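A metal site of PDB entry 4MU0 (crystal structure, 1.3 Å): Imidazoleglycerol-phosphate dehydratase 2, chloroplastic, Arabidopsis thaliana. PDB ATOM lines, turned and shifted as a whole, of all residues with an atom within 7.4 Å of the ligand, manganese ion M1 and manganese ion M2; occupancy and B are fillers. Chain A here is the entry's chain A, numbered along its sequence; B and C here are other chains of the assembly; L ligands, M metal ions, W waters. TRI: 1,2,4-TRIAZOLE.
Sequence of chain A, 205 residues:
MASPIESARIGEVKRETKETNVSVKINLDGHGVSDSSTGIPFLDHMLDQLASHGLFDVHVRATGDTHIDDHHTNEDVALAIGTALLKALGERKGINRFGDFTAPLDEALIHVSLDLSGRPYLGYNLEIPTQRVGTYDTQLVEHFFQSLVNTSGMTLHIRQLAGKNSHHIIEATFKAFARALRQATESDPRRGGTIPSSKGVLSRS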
ATOM      1  N   GLU A  19      32.231   9.414 -25.119  1.00  0.00           N
ATOM      2  CA  GLU A  19      31.618  10.477 -24.300  1.00  0.00           C
ATOM      3  C   GLU A  19      32.423  10.904 -23.052  1.00  0.00           C
ATOM      4  O   GLU A  19      32.350  12.042 -22.647  1.00  0.00           O
ATOM      5  CB  GLU A  19      30.193  10.032 -23.859  1.00  0.00           C
ATOM      6  CG  GLU A  19      29.186   9.832 -25.014  1.00  0.00           C
ATOM      7  CD  GLU A  19      29.274   8.474 -25.670  1.00  0.00           C
ATOM      8  OE1 GLU A  19      29.822   7.542 -25.035  1.00  0.00           O
ATOM      9  OE2 GLU A  19      28.786   8.332 -26.815  1.00  0.00           O
ATOM     10  N   ASP A  65      31.518  14.927 -21.592  1.00  0.00           N
ATOM     11  CA  ASP A  65      30.718  15.821 -22.446  1.00  0.00           C
ATOM     12  C   ASP A  65      29.681  16.640 -21.693  1.00  0.00           C
ATOM     13  O   ASP A  65      28.501  16.666 -22.025  1.00  0.00           O
ATOM     14  CB  ASP A  65      30.130  15.058 -23.629  1.00  0.00           C
ATOM     15  CG  ASP A  65      29.230  13.876 -23.214  1.00  0.00           C
ATOM     16  OD1 ASP A  65      28.981  13.664 -22.020  1.00  0.00           O
ATOM     17  OD2 ASP A  65      28.756  13.167 -24.129  1.00  0.00           O
ATOM     18  N   ILE A  68      26.902  18.891 -23.128  1.00  0.00           N
ATOM     19  CA  ILE A  68      25.618  18.292 -23.475  1.00  0.00           C
ATOM     20  C   ILE A  68      24.725  18.219 -22.248  1.00  0.00           C
ATOM     21  O   ILE A  68      23.604  18.664 -22.290  1.00  0.00           O
ATOM     22  CB  ILE A  68      25.811  16.888 -24.074  1.00  0.00           C
ATOM     23  CG1 ILE A  68      26.563  16.951 -25.375  1.00  0.00           C
ATOM     24  CG2 ILE A  68      24.473  16.184 -24.264  1.00  0.00           C
ATOM     25  CD1 ILE A  68      26.949  15.599 -25.895  1.00  0.00           C
ATOM     26  N   ASP A  69      25.245  17.590 -21.209  1.00  0.00           N
ATOM     27  CA  ASP A  69      24.724  17.660 -19.854  1.00  0.00           C
ATOM     28  C   ASP A  69      25.590  16.771 -18.997  1.00  0.00           C
ATOM     29  O   ASP A  69      26.549  16.189 -19.495  1.00  0.00           O
ATOM     30  CB  ASP A  69      23.236  17.376 -19.697  1.00  0.00           C
ATOM     31  CG  ASP A  69      22.868  15.932 -19.900  1.00  0.00           C
ATOM     32  OD1 ASP A  69      23.770  15.188 -20.215  1.00  0.00           O
ATOM     33  OD2 ASP A  69      21.654  15.499 -19.747  1.00  0.00           O
ATOM     34  N   HIS A  71      24.848  14.052 -17.614  1.00  0.00           N
ATOM     35  CA  HIS A  71      24.338  12.689 -17.575  1.00  0.00           C
ATOM     36  C   HIS A  71      25.382  11.626 -17.899  1.00  0.00           C
ATOM     37  O   HIS A  71      25.533  10.647 -17.152  1.00  0.00           O
ATOM     38  CB  HIS A  71      23.176  12.581 -18.558  1.00  0.00           C
ATOM     39  CG  HIS A  71      22.437  11.287 -18.512  1.00  0.00           C
ATOM     40  ND1 HIS A  71      21.087  11.240 -18.315  1.00  0.00           N
ATOM     41  CD2 HIS A  71      22.827   9.995 -18.673  1.00  0.00           C
ATOM     42  CE1 HIS A  71      20.678   9.987 -18.352  1.00  0.00           C
ATOM     43  NE2 HIS A  71      21.707   9.205 -18.596  1.00  0.00           N
ATOM     44  N   HIS A  72      26.063  11.751 -19.050  1.00  0.00           N
ATOM     45  CA  HIS A  72      26.963  10.653 -19.416  1.00  0.00           C
ATOM     46  C   HIS A  72      28.110  10.505 -18.392  1.00  0.00           C
ATOM     47  O   HIS A  72      28.504   9.406 -18.046  1.00  0.00           O
ATOM     48  CB  HIS A  72      27.537  10.844 -20.832  1.00  0.00           C
ATOM     49  CG  HIS A  72      26.518  10.928 -21.929  1.00  0.00           C
ATOM     50  ND1 HIS A  72      26.764  11.612 -23.079  1.00  0.00           N
ATOM     51  CD2 HIS A  72      25.261  10.449 -22.062  1.00  0.00           C
ATOM     52  CE1 HIS A  72      25.726  11.545 -23.890  1.00  0.00           C
ATOM     53  NE2 HIS A  72      24.794  10.838 -23.299  1.00  0.00           N
ATOM     54  N   GLU A  75      26.795   8.912 -15.145  1.00  0.00           N
ATOM     55  CA  GLU A  75      26.562   7.501 -15.377  1.00  0.00           C
ATOM     56  C   GLU A  75      27.849   6.696 -15.431  1.00  0.00           C
ATOM     57  O   GLU A  75      27.974   5.637 -14.806  1.00  0.00           O
ATOM     58  CB  GLU A  75      25.775   7.333 -16.688  1.00  0.00           C
ATOM     59  CG  GLU A  75      25.554   5.881 -17.086  1.00  0.00           C
ATOM     60  CD  GLU A  75      24.478   5.671 -18.148  1.00  0.00           C
ATOM     61  OE1 GLU A  75      23.866   6.674 -18.563  1.00  0.00           O
ATOM     62  OE2 GLU A  75      24.207   4.487 -18.488  1.00  0.00           O
ATOM     63  N   LEU A 140      19.766  12.915 -11.678  1.00  0.00           N
ATOM     64  CA  LEU A 140      20.968  12.122 -11.813  1.00  0.00           C
ATOM     65  C   LEU A 140      21.315  11.328 -10.569  1.00  0.00           C
ATOM     66  O   LEU A 140      22.121  10.404 -10.629  1.00  0.00           O
ATOM     67  CB  LEU A 140      22.115  12.986 -12.297  1.00  0.00           C
ATOM     68  CG  LEU A 140      21.850  13.635 -13.657  1.00  0.00           C
ATOM     69  CD1 LEU A 140      23.058  14.467 -14.093  1.00  0.00           C
ATOM     70  CD2 LEU A 140      21.572  12.603 -14.742  1.00  0.00           C
ATOM     71  N   HIS A 143      20.013   7.838 -11.104  1.00  0.00           N
ATOM     72  CA  HIS A 143      20.825   7.178 -12.127  1.00  0.00           C
ATOM     73  C   HIS A 143      22.212   6.763 -11.609  1.00  0.00           C
ATOM     74  O   HIS A 143      22.721   5.713 -11.974  1.00  0.00           O
ATOM     75  CB  HIS A 143      20.976   8.076 -13.368  1.00  0.00           C
ATOM     76  CG  HIS A 143      21.230   7.333 -14.638  1.00  0.00           C
ATOM     77  ND1 HIS A 143      22.040   6.218 -14.728  1.00  0.00           N
ATOM     78  CD2 HIS A 143      20.849   7.596 -15.911  1.00  0.00           C
ATOM     79  CE1 HIS A 143      22.083   5.821 -15.993  1.00  0.00           C
ATOM     80  NE2 HIS A 143      21.372   6.648 -16.722  1.00  0.00           N
ATOM     81  N   SER A 147      23.198   2.808 -11.767  1.00  0.00           N
ATOM     82  CA  SER A 147      24.354   2.392 -12.505  1.00  0.00           C
ATOM     83  C   SER A 147      25.383   1.685 -11.600  1.00  0.00           C
ATOM     84  O   SER A 147      25.938   0.663 -11.959  1.00  0.00           O
ATOM     85  CB  SER A 147      24.965   3.601 -13.206  1.00  0.00           C
ATOM     86  OG  SER A 147      24.117   4.085 -14.229  1.00  0.00           O
ATOM     87  N   PHE B  42      22.779  19.773 -26.923  1.00  0.00           N
ATOM     88  CA  PHE B  42      21.900  18.633 -26.755  1.00  0.00           C
ATOM     89  C   PHE B  42      21.251  18.242 -28.110  1.00  0.00           C
ATOM     90  O   PHE B  42      21.052  17.063 -28.387  1.00  0.00           O
ATOM     91  CB  PHE B  42      20.819  18.837 -25.692  1.00  0.00           C
ATOM     92  CG  PHE B  42      20.143  17.551 -25.279  1.00  0.00           C
ATOM     93  CD1 PHE B  42      20.717  16.735 -24.357  1.00  0.00           C
ATOM     94  CD2 PHE B  42      18.959  17.156 -25.874  1.00  0.00           C
ATOM     95  CE1 PHE B  42      20.157  15.531 -24.002  1.00  0.00           C
ATOM     96  CE2 PHE B  42      18.400  15.930 -25.508  1.00  0.00           C
ATOM     97  CZ  PHE B  42      19.013  15.120 -24.597  1.00  0.00           C
ATOM     98  N   HIS B  45      23.612  16.266 -30.069  1.00  0.00           N
ATOM     99  CA  HIS B  45      23.640  14.873 -29.594  1.00  0.00           C
ATOM    100  C   HIS B  45      22.452  14.088 -30.184  1.00  0.00           C
ATOM    101  O   HIS B  45      22.598  12.935 -30.588  1.00  0.00           O
ATOM    102  CB  HIS B  45      23.650  14.911 -28.051  1.00  0.00           C
ATOM    103  CG  HIS B  45      23.656  13.566 -27.397  1.00  0.00           C
ATOM    104  ND1 HIS B  45      24.457  12.527 -27.822  1.00  0.00           N
ATOM    105  CD2 HIS B  45      23.026  13.106 -26.280  1.00  0.00           C
ATOM    106  CE1 HIS B  45      24.273  11.475 -27.019  1.00  0.00           C
ATOM    107  NE2 HIS B  45      23.405  11.803 -26.084  1.00  0.00           N
ATOM    108  N   MET B  46      21.289  14.689 -30.225  1.00  0.00           N
ATOM    109  CA  MET B  46      20.122  14.019 -30.807  1.00  0.00           C
ATOM    110  C   MET B  46      20.266  13.804 -32.309  1.00  0.00           C
ATOM    111  O   MET B  46      19.885  12.757 -32.824  1.00  0.00           O
ATOM    112  CB  MET B  46      18.837  14.792 -30.492  1.00  0.00           C
ATOM    113  CG  MET B  46      18.454  14.826 -29.028  1.00  0.00           C
ATOM    114  SD  MET B  46      18.350  13.192 -28.242  1.00  0.00           S
ATOM    115  CE  MET B  46      20.000  13.034 -27.501  1.00  0.00           C
ATOM    116  N   GLN B  49      22.245  10.846 -32.978  1.00  0.00           N
ATOM    117  CA  GLN B  49      21.434   9.627 -32.845  1.00  0.00           C
ATOM    118  C   GLN B  49      20.648   9.360 -34.108  1.00  0.00           C
ATOM    119  O   GLN B  49      20.480   8.223 -34.561  1.00  0.00           O
ATOM    120  CB  GLN B  49      20.477   9.690 -31.640  1.00  0.00           C
ATOM    121  CG  GLN B  49      21.142   9.927 -30.300  1.00  0.00           C
ATOM    122  CD  GLN B  49      22.276   9.012 -30.045  1.00  0.00           C
ATOM    123  OE1 GLN B  49      22.132   7.806 -30.179  1.00  0.00           O
ATOM    124  NE2 GLN B  49      23.426   9.555 -29.658  1.00  0.00           N
ATOM    125  N   LEU B 105      15.255   3.201 -23.998  1.00  0.00           N
ATOM    126  CA  LEU B 105      16.540   3.619 -23.484  1.00  0.00           C
ATOM    127  C   LEU B 105      16.350   3.470 -21.968  1.00  0.00           C
ATOM    128  O   LEU B 105      15.667   4.254 -21.320  1.00  0.00           O
ATOM    129  CB  LEU B 105      16.951   5.034 -23.852  1.00  0.00           C
ATOM    130  CG  LEU B 105      18.438   5.297 -23.592  1.00  0.00           C
ATOM    131  CD1 LEU B 105      18.789   6.701 -24.026  1.00  0.00           C
ATOM    132  CD2 LEU B 105      19.000   4.974 -22.251  1.00  0.00           C
ATOM    133  N   ASP B 106      16.877   2.373 -21.441  1.00  0.00           N
ATOM    134  CA  ASP B 106      16.680   1.989 -20.053  1.00  0.00           C
ATOM    135  C   ASP B 106      15.164   1.979 -19.760  1.00  0.00           C
ATOM    136  O   ASP B 106      14.422   1.236 -20.414  1.00  0.00           O
ATOM    137  CB  ASP B 106      17.528   2.814 -19.081  1.00  0.00           C
ATOM    138  CG  ASP B 106      19.012   2.645 -19.281  1.00  0.00           C
ATOM    139  OD1 ASP B 106      19.422   1.769 -20.066  1.00  0.00           O
ATOM    140  OD2 ASP B 106      19.749   3.385 -18.606  1.00  0.00           O
ATOM    141  N   GLU B 107      14.705   2.761 -18.779  1.00  0.00           N
ATOM    142  CA  GLU B 107      13.308   2.749 -18.353  1.00  0.00           C
ATOM    143  C   GLU B 107      12.383   3.438 -19.347  1.00  0.00           C
ATOM    144  O   GLU B 107      11.176   3.303 -19.246  1.00  0.00           O
ATOM    145  CB  GLU B 107      13.216   3.379 -16.965  1.00  0.00           C
ATOM    146  CG  GLU B 107      12.966   4.894 -16.887  1.00  0.00           C
ATOM    147  CD  GLU B 107      14.029   5.774 -17.516  1.00  0.00           C
ATOM    148  OE1 GLU B 107      15.180   5.327 -17.638  1.00  0.00           O
ATOM    149  OE2 GLU B 107      13.671   6.942 -17.865  1.00  0.00           O
ATOM    150  N   ASN B 165      13.533   9.609 -16.790  1.00  0.00           N
ATOM    151  CA  ASN B 165      14.683  10.471 -17.004  1.00  0.00           C
ATOM    152  C   ASN B 165      14.502  11.227 -18.311  1.00  0.00           C
ATOM    153  O   ASN B 165      14.259  10.629 -19.350  1.00  0.00           O
ATOM    154  CB  ASN B 165      15.953   9.635 -17.010  1.00  0.00           C
ATOM    155  CG  ASN B 165      17.185  10.500 -17.247  1.00  0.00           C
ATOM    156  OD1 ASN B 165      17.436  10.946 -18.373  1.00  0.00           O
ATOM    157  ND2 ASN B 165      17.884  10.806 -16.181  1.00  0.00           N
ATOM    158  N   HIS B 167      16.506  12.943 -20.332  1.00  0.00           N
ATOM    159  CA  HIS B 167      17.455  12.631 -21.383  1.00  0.00           C
ATOM    160  C   HIS B 167      17.110  11.281 -22.014  1.00  0.00           C
ATOM    161  O   HIS B 167      17.110  11.156 -23.232  1.00  0.00           O
ATOM    162  CB  HIS B 167      18.858  12.682 -20.764  1.00  0.00           C
ATOM    163  CG  HIS B 167      20.040  12.479 -21.679  1.00  0.00           C
ATOM    164  ND1 HIS B 167      21.219  13.182 -21.456  1.00  0.00           N
ATOM    165  CD2 HIS B 167      20.306  11.609 -22.674  1.00  0.00           C
ATOM    166  CE1 HIS B 167      22.138  12.753 -22.325  1.00  0.00           C
ATOM    167  NE2 HIS B 167      21.613  11.788 -23.055  1.00  0.00           N
ATOM    168  N   HIS B 168      16.775  10.297 -21.205  1.00  0.00           N
ATOM    169  CA  HIS B 168      16.355   9.009 -21.736  1.00  0.00           C
ATOM    170  C   HIS B 168      15.119   9.115 -22.629  1.00  0.00           C
ATOM    171  O   HIS B 168      15.041   8.508 -23.691  1.00  0.00           O
ATOM    172  CB  HIS B 168      16.098   7.979 -20.655  1.00  0.00           C
ATOM    173  CG  HIS B 168      17.334   7.547 -19.918  1.00  0.00           C
ATOM    174  ND1 HIS B 168      17.292   6.691 -18.855  1.00  0.00           N
ATOM    175  CD2 HIS B 168      18.639   7.824 -20.128  1.00  0.00           C
ATOM    176  CE1 HIS B 168      18.527   6.435 -18.431  1.00  0.00           C
ATOM    177  NE2 HIS B 168      19.364   7.122 -19.182  1.00  0.00           N
ATOM    178  N   GLU B 171      16.068  10.973 -25.937  1.00  0.00           N
ATOM    179  CA  GLU B 171      16.985  10.184 -26.752  1.00  0.00           C
ATOM    180  C   GLU B 171      16.302   8.954 -27.328  1.00  0.00           C
ATOM    181  O   GLU B 171      16.484   8.653 -28.523  1.00  0.00           O
ATOM    182  CB  GLU B 171      18.258   9.853 -26.011  1.00  0.00           C
ATOM    183  CG  GLU B 171      19.302   9.216 -26.902  1.00  0.00           C
ATOM    184  CD  GLU B 171      20.658   9.075 -26.290  1.00  0.00           C
ATOM    185  OE1 GLU B 171      20.996   9.916 -25.459  1.00  0.00           O
ATOM    186  OE2 GLU B 171      21.353   8.063 -26.583  1.00  0.00           O
ATOM    187  N   LYS B 175      15.916   7.799 -31.254  1.00  0.00           N
ATOM    188  CA  LYS B 175      16.265   6.472 -31.713  1.00  0.00           C
ATOM    189  C   LYS B 175      15.093   5.842 -32.484  1.00  0.00           C
ATOM    190  O   LYS B 175      15.260   5.281 -33.564  1.00  0.00           O
ATOM    191  CB  LYS B 175      16.663   5.531 -30.579  1.00  0.00           C
ATOM    192  CG  LYS B 175      17.980   5.945 -29.928  1.00  0.00           C
ATOM    193  CD  LYS B 175      18.392   5.041 -28.768  1.00  0.00           C
ATOM    194  CE  LYS B 175      19.715   5.511 -28.092  1.00  0.00           C
ATOM    195  NZ  LYS B 175      20.298   4.504 -27.181  1.00  0.00           N
ATOM    196  N   ARG C 119      23.136  -2.670 -20.506  1.00  0.00           N
ATOM    197  CA  ARG C 119      22.624  -2.105 -19.258  1.00  0.00           C
ATOM    198  C   ARG C 119      21.351  -2.885 -18.890  1.00  0.00           C
ATOM    199  O   ARG C 119      20.388  -2.848 -19.646  1.00  0.00           O
ATOM    200  CB  ARG C 119      22.258  -0.646 -19.457  1.00  0.00           C
ATOM    201  CG  ARG C 119      23.429   0.232 -19.803  1.00  0.00           C
ATOM    202  CD  ARG C 119      23.018   1.691 -19.928  1.00  0.00           C
ATOM    203  NE  ARG C 119      22.079   1.871 -21.000  1.00  0.00           N
ATOM    204  CZ  ARG C 119      22.410   2.183 -22.233  1.00  0.00           C
ATOM    205  NH1 ARG C 119      23.670   2.448 -22.575  1.00  0.00           N
ATOM    206  NH2 ARG C 119      21.481   2.252 -23.167  1.00  0.00           N
HETATM  207  N1  TRI L   1      22.405   8.660 -22.972  1.00  0.00           N
HETATM  208  N2  TRI L   1      22.659   7.340 -23.250  1.00  0.00           N
HETATM  209  C3  TRI L   1      22.408   6.686 -22.080  1.00  0.00           C
HETATM  210  N4  TRI L   1      22.058   7.526 -21.143  1.00  0.00           N
HETATM  211  C5  TRI L   1      22.022   8.747 -21.698  1.00  0.00           C
HETATM  212 MN    MN M   1      22.841  10.361 -24.394  1.00  0.00          MN
HETATM  213 MN    MN M   2      21.633   6.992 -18.998  1.00  0.00          MN
HETATM  214  O   HOH W   1      21.762   4.890 -19.545  1.00  0.00           O
HETATM  215  O   HOH W   2      23.835   8.740 -25.656  1.00  0.00           O
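The backbone NH (N) of His 71 is in hydrogen-bond range of the side-chain carboxylate (OD1) of Asp 69 (3.0 Å).
The side-chain amide oxygen of Asn 165 of chain B is in hydrogen-bond range of the backbone NH of His 168 of chain B, 3.0 Å away.
A ring nitrogen (ND1) of His 168 of chain B is in hydrogen-bond range of the side-chain carboxylate (OE1) of Glu 107 of chain B (2.8 Å).
ND1 of His 72 lies within hydrogen-bond range of OD2 of Asp 65 (2.7 Å).
N of His 167 of chain B lies within hydrogen-bond range of OD1 of Asn 165 of chain B, 2.9 Å away.
The side-chain carboxylate of Asp 69 sits at hydrogen-bond distance from a ring nitrogen (ND1) of His 167 of chain B, 2.9 Å away.
The side-chain hydroxyl (OG) of Ser 147 lies within hydrogen-bond range of a ring nitrogen (ND1) of His 143.
Merely in contact with the ligand: Leu 105 of chain B (3.8 Å).
Hydrophobic or aromatic side chains that line the ligand: His 71, His 72, Leu 105 of chain B, His 167 of chain B and His 168 of chain B.
Within 4 Å of the ligand: His 71, His 72, Glu 75, Leu 105 of chain B, His 167 of chain B, His 168 of chain B and Glu 171 of chain B.
The nearest printed residue that does not touch the ligand is Arg 119 of chain C (4.4 Å).
The nearest printed residue that does not touch manganese ion M1 is Met 46 of chain B (5.0 Å).
Within 4 Å of manganese ion M2: His 71, Glu 75, His 143 and His 168 of chain B.
The nearest printed residue that does not touch manganese ion M2 is Asp 106 of chain B (4.1 Å).
Manganese ion M1 is bound by OE1 of Glu 171 of chain B (2.2 Å), N1 of the ligand (2.3 Å), water W2 (2.3 Å), NE2 of His 72 (2.3 Å), NE2 of His 45 of chain B (2.3 Å) and NE2 of His 167 of chain B (2.3 Å).
Water W1 binds manganese ion M2 (2.2 Å).
A ring nitrogen (NE2) of His 71 is bound to manganese ion M2.
N4 of the ligand binds manganese ion M2 (2.3 Å).
NE2 of His 168 of chain B binds manganese ion M2 (2.3 Å).
Manganese ion M2 is bound by OE1 of Glu 75.
A ring nitrogen (NE2) of His 143 is bound to manganese ion M2 (2.3 Å).
Water W2 bridges OE2 of Glu 171 of chain B and N2 of the ligand.
Water W1 lies within hydrogen-bond range of the side-chain carboxylate of Asp 106 of chain B (2.7 Å), the side-chain carboxylate of Glu 75 (2.7 Å) and the guanidinium group of Arg 119 of chain C (3.4 Å).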
